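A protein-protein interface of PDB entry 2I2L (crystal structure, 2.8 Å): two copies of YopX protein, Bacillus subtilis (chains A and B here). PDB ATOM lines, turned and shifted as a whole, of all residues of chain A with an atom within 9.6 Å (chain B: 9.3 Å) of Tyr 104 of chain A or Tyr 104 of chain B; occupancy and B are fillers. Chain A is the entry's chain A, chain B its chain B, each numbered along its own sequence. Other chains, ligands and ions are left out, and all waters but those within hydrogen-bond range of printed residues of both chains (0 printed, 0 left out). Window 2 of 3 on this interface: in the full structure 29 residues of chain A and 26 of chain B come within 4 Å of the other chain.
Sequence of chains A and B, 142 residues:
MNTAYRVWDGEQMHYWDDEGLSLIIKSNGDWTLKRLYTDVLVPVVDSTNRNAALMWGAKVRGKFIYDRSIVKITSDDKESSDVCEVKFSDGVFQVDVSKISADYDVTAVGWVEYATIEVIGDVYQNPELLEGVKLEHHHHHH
The side-chain hydroxyl of Tyr 104 of chain A is in hydrogen-bond range of the side-chain hydroxyl of Tyr 104 of chain B (3.5 Å).
The backbone NH (N) of Val 95 of chain A lies within hydrogen-bond range of the backbone carbonyl oxygen (O) of Thr 107 of chain A. The backbone carbonyl oxygen (O) of Thr 107 of chain B sits at hydrogen-bond distance from the backbone NH (N) of Val 95 of chain B (2.9 Å).
CA of Thr 107 of chain A touches CH2 of Trp 111 of chain B, at 3.6 Å. Trp 111 of chain B touches Ala 108 of chain A. Trp 111 of chain A touches Thr 107 of chain B. Ala 108 of chain B touches Trp 111 of chain A.
Of chain A, only Tyr 104 (3.5 Å) comes within 4 Å of Tyr 104 of chain B. No residue of chain A comes within 4 Å of Val 97 of chain B. No residue of chain A comes within 4 Å of Asp 103 of chain B. Asp 105 of chain B touches none of the printed residues of chain A. Printed residues of chain B within 4 Å of Ala 108 of chain A: Trp 111. Printed residues of chain B within 4 Å of Thr 107 of chain A: Trp 111 (3.6 Å). Printed residues of chain A within 4 Å of Thr 107 of chain B: Trp 111. Of the printed residues of chain B, Trp 111 of chain A touches Thr 107 (3.8 Å) and Ala 108 (3.7 Å). Lys 99 of chain A touches none of the printed residues of chain B. The nearest printed residue of chain A that does not touch Trp 111 of chain B is Trp 111 of chain A (4.3 Å).
Of the 15 printed residues of chain A, 4 touch a printed residue of chain B. Hydrophobic or aromatic side chains of chain A within 4 Å of the printed part of chain B: Tyr 104 and Trp 111. Of the 15 printed residues of chain B, 4 touch a printed residue of chain A. Among the printed residues, no Asp or Glu carboxylate lies within 4 Å of a Lys or Arg side-chain nitrogen of the other chain.
Tyr 104 of chain B touches its own counterpart, Tyr 104 of chain A. Thr 107 of chain A touches Trp 111 of chain B, and with the chains exchanged Trp 111 of chain A touches Thr 107 of chain B. Ala 108 of chain A touches Trp 111 of chain B, and with the chains exchanged Trp 111 of chain A touches Ala 108 of chain B. Positions printed for both chains: 95, 96, 97, 98, 99, 104, 105, 106, 107, 108, 111, 112, 113 and 114.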
ATOM      1  N   ASP A  82      16.225  25.142 -26.553  1.00  0.00           N
ATOM      2  CA  ASP A  82      16.028  26.545 -26.221  1.00  0.00           C
ATOM      3  C   ASP A  82      15.780  26.676 -24.731  1.00  0.00           C
ATOM      4  O   ASP A  82      15.636  25.684 -24.011  1.00  0.00           O
ATOM      5  CB  ASP A  82      14.825  27.099 -27.001  1.00  0.00           C
ATOM      6  CG  ASP A  82      14.804  28.619 -27.067  1.00  0.00           C
ATOM      7  OD1 ASP A  82      15.605  29.281 -26.371  1.00  0.00           O
ATOM      8  OD2 ASP A  82      13.969  29.161 -27.823  1.00  0.00           O
ATOM      9  N   VAL A  95       4.606  28.143 -23.759  1.00  0.00           N
ATOM     10  CA  VAL A  95       6.045  28.340 -23.915  1.00  0.00           C
ATOM     11  C   VAL A  95       6.374  28.649 -25.370  1.00  0.00           C
ATOM     12  O   VAL A  95       5.650  28.227 -26.271  1.00  0.00           O
ATOM     13  CB  VAL A  95       6.825  27.076 -23.486  1.00  0.00           C
ATOM     14  CG1 VAL A  95       6.512  25.930 -24.418  1.00  0.00           C
ATOM     15  CG2 VAL A  95       8.310  27.357 -23.473  1.00  0.00           C
ATOM     16  N   ASP A  96       7.455  29.391 -25.599  1.00  0.00           N
ATOM     17  CA  ASP A  96       7.856  29.733 -26.960  1.00  0.00           C
ATOM     18  C   ASP A  96       8.367  28.494 -27.684  1.00  0.00           C
ATOM     19  O   ASP A  96       9.389  27.923 -27.320  1.00  0.00           O
ATOM     20  CB  ASP A  96       8.937  30.826 -26.951  1.00  0.00           C
ATOM     21  CG  ASP A  96       9.701  30.926 -28.288  1.00  0.00           C
ATOM     22  OD1 ASP A  96       9.062  30.975 -29.366  1.00  0.00           O
ATOM     23  OD2 ASP A  96      10.952  30.963 -28.252  1.00  0.00           O
ATOM     24  N   VAL A  97       7.649  28.070 -28.713  1.00  0.00           N
ATOM     25  CA  VAL A  97       8.072  26.888 -29.440  1.00  0.00           C
ATOM     26  C   VAL A  97       8.566  27.159 -30.851  1.00  0.00           C
ATOM     27  O   VAL A  97       8.228  26.431 -31.786  1.00  0.00           O
ATOM     28  CB  VAL A  97       6.955  25.817 -29.479  1.00  0.00           C
ATOM     29  CG1 VAL A  97       6.916  25.073 -28.147  1.00  0.00           C
ATOM     30  CG2 VAL A  97       5.604  26.471 -29.766  1.00  0.00           C
ATOM     31  N   SER A  98       9.364  28.216 -30.995  1.00  0.00           N
ATOM     32  CA  SER A  98       9.959  28.563 -32.279  1.00  0.00           C
ATOM     33  C   SER A  98      11.253  27.748 -32.299  1.00  0.00           C
ATOM     34  O   SER A  98      12.369  28.286 -32.355  1.00  0.00           O
ATOM     35  CB  SER A  98      10.263  30.058 -32.338  1.00  0.00           C
ATOM     36  OG  SER A  98       9.101  30.821 -32.079  1.00  0.00           O
ATOM     37  N   LYS A  99      11.065  26.431 -32.210  1.00  0.00           N
ATOM     38  CA  LYS A  99      12.146  25.455 -32.189  1.00  0.00           C
ATOM     39  C   LYS A  99      11.571  24.098 -31.769  1.00  0.00           C
ATOM     40  O   LYS A  99      11.099  23.928 -30.641  1.00  0.00           O
ATOM     41  CB  LYS A  99      13.233  25.894 -31.206  1.00  0.00           C
ATOM     42  N   TYR A 104       4.819  25.930 -34.113  1.00  0.00           N
ATOM     43  CA  TYR A 104       4.165  27.214 -33.868  1.00  0.00           C
ATOM     44  C   TYR A 104       5.145  28.195 -33.231  1.00  0.00           C
ATOM     45  O   TYR A 104       6.344  28.161 -33.497  1.00  0.00           O
ATOM     46  CB  TYR A 104       2.969  27.045 -32.925  1.00  0.00           C
ATOM     47  CG  TYR A 104       2.042  25.892 -33.237  1.00  0.00           C
ATOM     48  CD1 TYR A 104       2.457  24.572 -33.072  1.00  0.00           C
ATOM     49  CD2 TYR A 104       0.732  26.125 -33.650  1.00  0.00           C
ATOM     50  CE1 TYR A 104       1.587  23.512 -33.308  1.00  0.00           C
ATOM     51  CE2 TYR A 104      -0.148  25.076 -33.891  1.00  0.00           C
ATOM     52  CZ  TYR A 104       0.283  23.773 -33.716  1.00  0.00           C
ATOM     53  OH  TYR A 104      -0.591  22.734 -33.936  1.00  0.00           O
ATOM     54  N   ASP A 105       4.613  29.072 -32.387  1.00  0.00           N
ATOM     55  CA  ASP A 105       5.412  30.059 -31.675  1.00  0.00           C
ATOM     56  C   ASP A 105       5.179  29.863 -30.185  1.00  0.00           C
ATOM     57  O   ASP A 105       6.099  29.989 -29.377  1.00  0.00           O
ATOM     58  CB  ASP A 105       4.992  31.474 -32.067  1.00  0.00           C
ATOM     59  CG  ASP A 105       5.493  31.870 -33.434  1.00  0.00           C
ATOM     60  OD1 ASP A 105       5.247  33.032 -33.830  1.00  0.00           O
ATOM     61  OD2 ASP A 105       6.133  31.023 -34.106  1.00  0.00           O
ATOM     62  N   VAL A 106       3.931  29.561 -29.839  1.00  0.00           N
ATOM     63  CA  VAL A 106       3.536  29.332 -28.459  1.00  0.00           C
ATOM     64  C   VAL A 106       2.608  28.124 -28.428  1.00  0.00           C
ATOM     65  O   VAL A 106       1.877  27.880 -29.383  1.00  0.00           O
ATOM     66  CB  VAL A 106       2.793  30.556 -27.885  1.00  0.00           C
ATOM     67  CG1 VAL A 106       3.710  31.770 -27.880  1.00  0.00           C
ATOM     68  CG2 VAL A 106       1.553  30.838 -28.713  1.00  0.00           C
ATOM     69  N   THR A 107       2.648  27.370 -27.335  1.00  0.00           N
ATOM     70  CA  THR A 107       1.801  26.190 -27.195  1.00  0.00           C
ATOM     71  C   THR A 107       1.819  25.706 -25.755  1.00  0.00           C
ATOM     72  O   THR A 107       2.750  25.996 -25.007  1.00  0.00           O
ATOM     73  CB  THR A 107       2.283  25.037 -28.111  1.00  0.00           C
ATOM     74  OG1 THR A 107       1.396  23.919 -27.981  1.00  0.00           O
ATOM     75  CG2 THR A 107       3.680  24.594 -27.722  1.00  0.00           C
ATOM     76  N   ALA A 108       0.789  24.970 -25.363  1.00  0.00           N
ATOM     77  CA  ALA A 108       0.727  24.453 -24.007  1.00  0.00           C
ATOM     78  C   ALA A 108       2.009  23.684 -23.764  1.00  0.00           C
ATOM     79  O   ALA A 108       2.535  23.068 -24.682  1.00  0.00           O
ATOM     80  CB  ALA A 108      -0.476  23.535 -23.849  1.00  0.00           C
ATOM     81  N   TRP A 111       1.521  20.131 -24.329  1.00  0.00           N
ATOM     82  CA  TRP A 111       1.180  19.799 -25.711  1.00  0.00           C
ATOM     83  C   TRP A 111       2.418  19.841 -26.605  1.00  0.00           C
ATOM     84  O   TRP A 111       2.304  19.786 -27.830  1.00  0.00           O
ATOM     85  CB  TRP A 111       0.113  20.762 -26.259  1.00  0.00           C
ATOM     86  CG  TRP A 111      -1.244  20.567 -25.641  1.00  0.00           C
ATOM     87  CD1 TRP A 111      -1.587  19.649 -24.676  1.00  0.00           C
ATOM     88  CD2 TRP A 111      -2.430  21.330 -25.905  1.00  0.00           C
ATOM     89  NE1 TRP A 111      -2.907  19.802 -24.325  1.00  0.00           N
ATOM     90  CE2 TRP A 111      -3.447  20.823 -25.058  1.00  0.00           C
ATOM     91  CE3 TRP A 111      -2.728  22.393 -26.764  1.00  0.00           C
ATOM     92  CZ2 TRP A 111      -4.747  21.350 -25.054  1.00  0.00           C
ATOM     93  CZ3 TRP A 111      -4.022  22.915 -26.757  1.00  0.00           C
ATOM     94  CH2 TRP A 111      -5.012  22.393 -25.904  1.00  0.00           C
ATOM     95  N   VAL A 112       3.597  19.964 -25.997  1.00  0.00           N
ATOM     96  CA  VAL A 112       4.833  19.979 -26.773  1.00  0.00           C
ATOM     97  C   VAL A 112       4.826  18.605 -27.416  1.00  0.00           C
ATOM     98  O   VAL A 112       4.860  17.588 -26.717  1.00  0.00           O
ATOM     99  CB  VAL A 112       6.041  20.132 -25.862  1.00  0.00           C
ATOM    100  N   GLU A 113       4.754  18.575 -28.742  1.00  0.00           N
ATOM    101  CA  GLU A 113       4.698  17.311 -29.472  1.00  0.00           C
ATOM    102  C   GLU A 113       6.035  16.587 -29.647  1.00  0.00           C
ATOM    103  O   GLU A 113       6.328  15.624 -28.928  1.00  0.00           O
ATOM    104  CB  GLU A 113       4.037  17.532 -30.840  1.00  0.00           C
ATOM    105  N   TYR A 114       6.844  17.050 -30.597  1.00  0.00           N
ATOM    106  CA  TYR A 114       8.121  16.405 -30.891  1.00  0.00           C
ATOM    107  C   TYR A 114       9.292  16.887 -30.047  1.00  0.00           C
ATOM    108  O   TYR A 114      10.411  17.012 -30.549  1.00  0.00           O
ATOM    109  CB  TYR A 114       8.447  16.576 -32.368  1.00  0.00           C
ATOM    110  N   VAL B  95     -11.339  23.005 -24.385  1.00  0.00           N
ATOM    111  CA  VAL B  95     -12.761  22.859 -24.680  1.00  0.00           C
ATOM    112  C   VAL B  95     -12.893  22.137 -26.014  1.00  0.00           C
ATOM    113  O   VAL B  95     -12.121  22.396 -26.950  1.00  0.00           O
ATOM    114  CB  VAL B  95     -13.464  24.227 -24.784  1.00  0.00           C
ATOM    115  CG1 VAL B  95     -12.847  25.053 -25.908  1.00  0.00           C
ATOM    116  CG2 VAL B  95     -14.948  24.022 -25.023  1.00  0.00           C
ATOM    117  N   ASP B  96     -13.862  21.228 -26.104  1.00  0.00           N
ATOM    118  CA  ASP B  96     -14.057  20.475 -27.338  1.00  0.00           C
ATOM    119  C   ASP B  96     -14.434  21.378 -28.496  1.00  0.00           C
ATOM    120  O   ASP B  96     -15.338  22.202 -28.381  1.00  0.00           O
ATOM    121  CB  ASP B  96     -15.135  19.408 -27.161  1.00  0.00           C
ATOM    122  CG  ASP B  96     -15.492  18.727 -28.472  1.00  0.00           C
ATOM    123  OD1 ASP B  96     -16.107  19.390 -29.337  1.00  0.00           O
ATOM    124  OD2 ASP B  96     -15.146  17.536 -28.645  1.00  0.00           O
ATOM    125  N   VAL B  97     -13.730  21.228 -29.611  1.00  0.00           N
ATOM    126  CA  VAL B  97     -14.007  22.027 -30.793  1.00  0.00           C
ATOM    127  C   VAL B  97     -14.329  21.103 -31.952  1.00  0.00           C
ATOM    128  O   VAL B  97     -14.556  21.559 -33.070  1.00  0.00           O
ATOM    129  CB  VAL B  97     -12.803  22.922 -31.180  1.00  0.00           C
ATOM    130  CG1 VAL B  97     -12.808  24.202 -30.358  1.00  0.00           C
ATOM    131  CG2 VAL B  97     -11.510  22.168 -30.953  1.00  0.00           C
ATOM    132  N   SER B  98     -14.360  19.803 -31.663  1.00  0.00           N
ATOM    133  CA  SER B  98     -14.641  18.773 -32.662  1.00  0.00           C
ATOM    134  C   SER B  98     -15.745  19.133 -33.655  1.00  0.00           C
ATOM    135  O   SER B  98     -15.782  18.593 -34.759  1.00  0.00           O
ATOM    136  CB  SER B  98     -14.977  17.452 -31.971  1.00  0.00           C
ATOM    137  N   LYS B  99     -16.643  20.037 -33.276  1.00  0.00           N
ATOM    138  CA  LYS B  99     -17.725  20.431 -34.174  1.00  0.00           C
ATOM    139  C   LYS B  99     -17.853  21.953 -34.280  1.00  0.00           C
ATOM    140  O   LYS B  99     -17.317  22.576 -35.199  1.00  0.00           O
ATOM    141  CB  LYS B  99     -19.045  19.820 -33.699  1.00  0.00           C
ATOM    142  N   ASP B 103     -10.430  21.041 -37.955  1.00  0.00           N
ATOM    143  CA  ASP B 103      -9.243  20.187 -37.903  1.00  0.00           C
ATOM    144  C   ASP B 103      -8.626  20.117 -36.498  1.00  0.00           C
ATOM    145  O   ASP B 103      -7.434  19.846 -36.340  1.00  0.00           O
ATOM    146  CB  ASP B 103      -8.204  20.673 -38.928  1.00  0.00           C
ATOM    147  CG  ASP B 103      -7.790  22.127 -38.711  1.00  0.00           C
ATOM    148  OD1 ASP B 103      -7.500  22.819 -39.713  1.00  0.00           O
ATOM    149  OD2 ASP B 103      -7.741  22.575 -37.546  1.00  0.00           O
ATOM    150  N   TYR B 104      -9.455  20.364 -35.486  1.00  0.00           N
ATOM    151  CA  TYR B 104      -9.033  20.324 -34.090  1.00  0.00           C
ATOM    152  C   TYR B 104     -10.076  19.598 -33.241  1.00  0.00           C
ATOM    153  O   TYR B 104     -11.271  19.827 -33.395  1.00  0.00           O
ATOM    154  CB  TYR B 104      -8.863  21.743 -33.537  1.00  0.00           C
ATOM    155  CG  TYR B 104      -7.508  22.367 -33.761  1.00  0.00           C
ATOM    156  CD1 TYR B 104      -6.338  21.641 -33.532  1.00  0.00           C
ATOM    157  CD2 TYR B 104      -7.394  23.700 -34.152  1.00  0.00           C
ATOM    158  CE1 TYR B 104      -5.083  22.228 -33.690  1.00  0.00           C
ATOM    159  CE2 TYR B 104      -6.146  24.302 -34.311  1.00  0.00           C
ATOM    160  CZ  TYR B 104      -4.991  23.560 -34.080  1.00  0.00           C
ATOM    161  OH  TYR B 104      -3.752  24.146 -34.237  1.00  0.00           O
ATOM    162  N   ASP B 105      -9.632  18.725 -32.343  1.00  0.00           N
ATOM    163  CA  ASP B 105     -10.571  18.016 -31.478  1.00  0.00           C
ATOM    164  C   ASP B 105     -10.874  18.871 -30.259  1.00  0.00           C
ATOM    165  O   ASP B 105     -12.038  19.118 -29.925  1.00  0.00           O
ATOM    166  CB  ASP B 105      -9.993  16.676 -31.020  1.00  0.00           C
ATOM    167  CG  ASP B 105     -10.521  15.508 -31.829  1.00  0.00           C
ATOM    168  OD1 ASP B 105     -11.744  15.493 -32.114  1.00  0.00           O
ATOM    169  OD2 ASP B 105      -9.720  14.606 -32.166  1.00  0.00           O
ATOM    170  N   VAL B 106      -9.806  19.305 -29.598  1.00  0.00           N
ATOM    171  CA  VAL B 106      -9.896  20.147 -28.413  1.00  0.00           C
ATOM    172  C   VAL B 106      -8.831  21.213 -28.550  1.00  0.00           C
ATOM    173  O   VAL B 106      -7.832  21.011 -29.238  1.00  0.00           O
ATOM    174  CB  VAL B 106      -9.596  19.360 -27.135  1.00  0.00           C
ATOM    175  CG1 VAL B 106     -10.569  18.214 -26.988  1.00  0.00           C
ATOM    176  CG2 VAL B 106      -8.181  18.846 -27.176  1.00  0.00           C
ATOM    177  N   THR B 107      -9.042  22.345 -27.897  1.00  0.00           N
ATOM    178  CA  THR B 107      -8.069  23.419 -27.950  1.00  0.00           C
ATOM    179  C   THR B 107      -8.244  24.305 -26.724  1.00  0.00           C
ATOM    180  O   THR B 107      -9.177  24.117 -25.944  1.00  0.00           O
ATOM    181  CB  THR B 107      -8.230  24.243 -29.254  1.00  0.00           C
ATOM    182  OG1 THR B 107      -7.194  25.228 -29.335  1.00  0.00           O
ATOM    183  CG2 THR B 107      -9.578  24.929 -29.291  1.00  0.00           C
ATOM    184  N   ALA B 108      -7.329  25.247 -26.533  1.00  0.00           N
ATOM    185  CA  ALA B 108      -7.417  26.159 -25.404  1.00  0.00           C
ATOM    186  C   ALA B 108      -8.592  27.089 -25.656  1.00  0.00           C
ATOM    187  O   ALA B 108      -8.722  27.636 -26.750  1.00  0.00           O
ATOM    188  CB  ALA B 108      -6.137  26.963 -25.283  1.00  0.00           C
ATOM    189  N   TRP B 111      -7.891  30.145 -27.207  1.00  0.00           N
ATOM    190  CA  TRP B 111      -7.271  30.003 -28.514  1.00  0.00           C
ATOM    191  C   TRP B 111      -8.289  29.631 -29.585  1.00  0.00           C
ATOM    192  O   TRP B 111      -7.912  29.286 -30.710  1.00  0.00           O
ATOM    193  CB  TRP B 111      -6.143  28.955 -28.474  1.00  0.00           C
ATOM    194  CG  TRP B 111      -4.919  29.400 -27.707  1.00  0.00           C
ATOM    195  CD1 TRP B 111      -4.654  30.662 -27.239  1.00  0.00           C
ATOM    196  CD2 TRP B 111      -3.786  28.598 -27.349  1.00  0.00           C
ATOM    197  NE1 TRP B 111      -3.429  30.692 -26.615  1.00  0.00           N
ATOM    198  CE2 TRP B 111      -2.874  29.437 -26.668  1.00  0.00           C
ATOM    199  CE3 TRP B 111      -3.451  27.253 -27.537  1.00  0.00           C
ATOM    200  CZ2 TRP B 111      -1.649  28.972 -26.173  1.00  0.00           C
ATOM    201  CZ3 TRP B 111      -2.233  26.790 -27.047  1.00  0.00           C
ATOM    202  CH2 TRP B 111      -1.349  27.649 -26.372  1.00  0.00           C
ATOM    203  N   VAL B 112      -9.575  29.685 -29.234  1.00  0.00           N
ATOM    204  CA  VAL B 112     -10.629  29.383 -30.202  1.00  0.00           C
ATOM    205  C   VAL B 112     -10.486  30.469 -31.272  1.00  0.00           C
ATOM    206  O   VAL B 112     -10.586  31.667 -30.973  1.00  0.00           O
ATOM    207  CB  VAL B 112     -12.004  29.457 -29.539  1.00  0.00           C
ATOM    208  N   GLU B 113     -10.253  30.054 -32.513  1.00  0.00           N
ATOM    209  CA  GLU B 113     -10.027  31.012 -33.595  1.00  0.00           C
ATOM    210  C   GLU B 113     -11.206  31.519 -34.421  1.00  0.00           C
ATOM    211  O   GLU B 113     -11.456  32.725 -34.452  1.00  0.00           O
ATOM    212  CB  GLU B 113      -8.936  30.466 -34.543  1.00  0.00           C
ATOM    213  N   TYR B 114     -11.922  30.613 -35.086  1.00  0.00           N
ATOM    214  CA  TYR B 114     -13.027  31.004 -35.969  1.00  0.00           C
ATOM    215  C   TYR B 114     -14.436  31.150 -35.394  1.00  0.00           C
ATOM    216  O   TYR B 114     -15.367  31.452 -36.136  1.00  0.00           O
ATOM    217  CB  TYR B 114     -13.067  30.056 -37.162  1.00  0.00           C
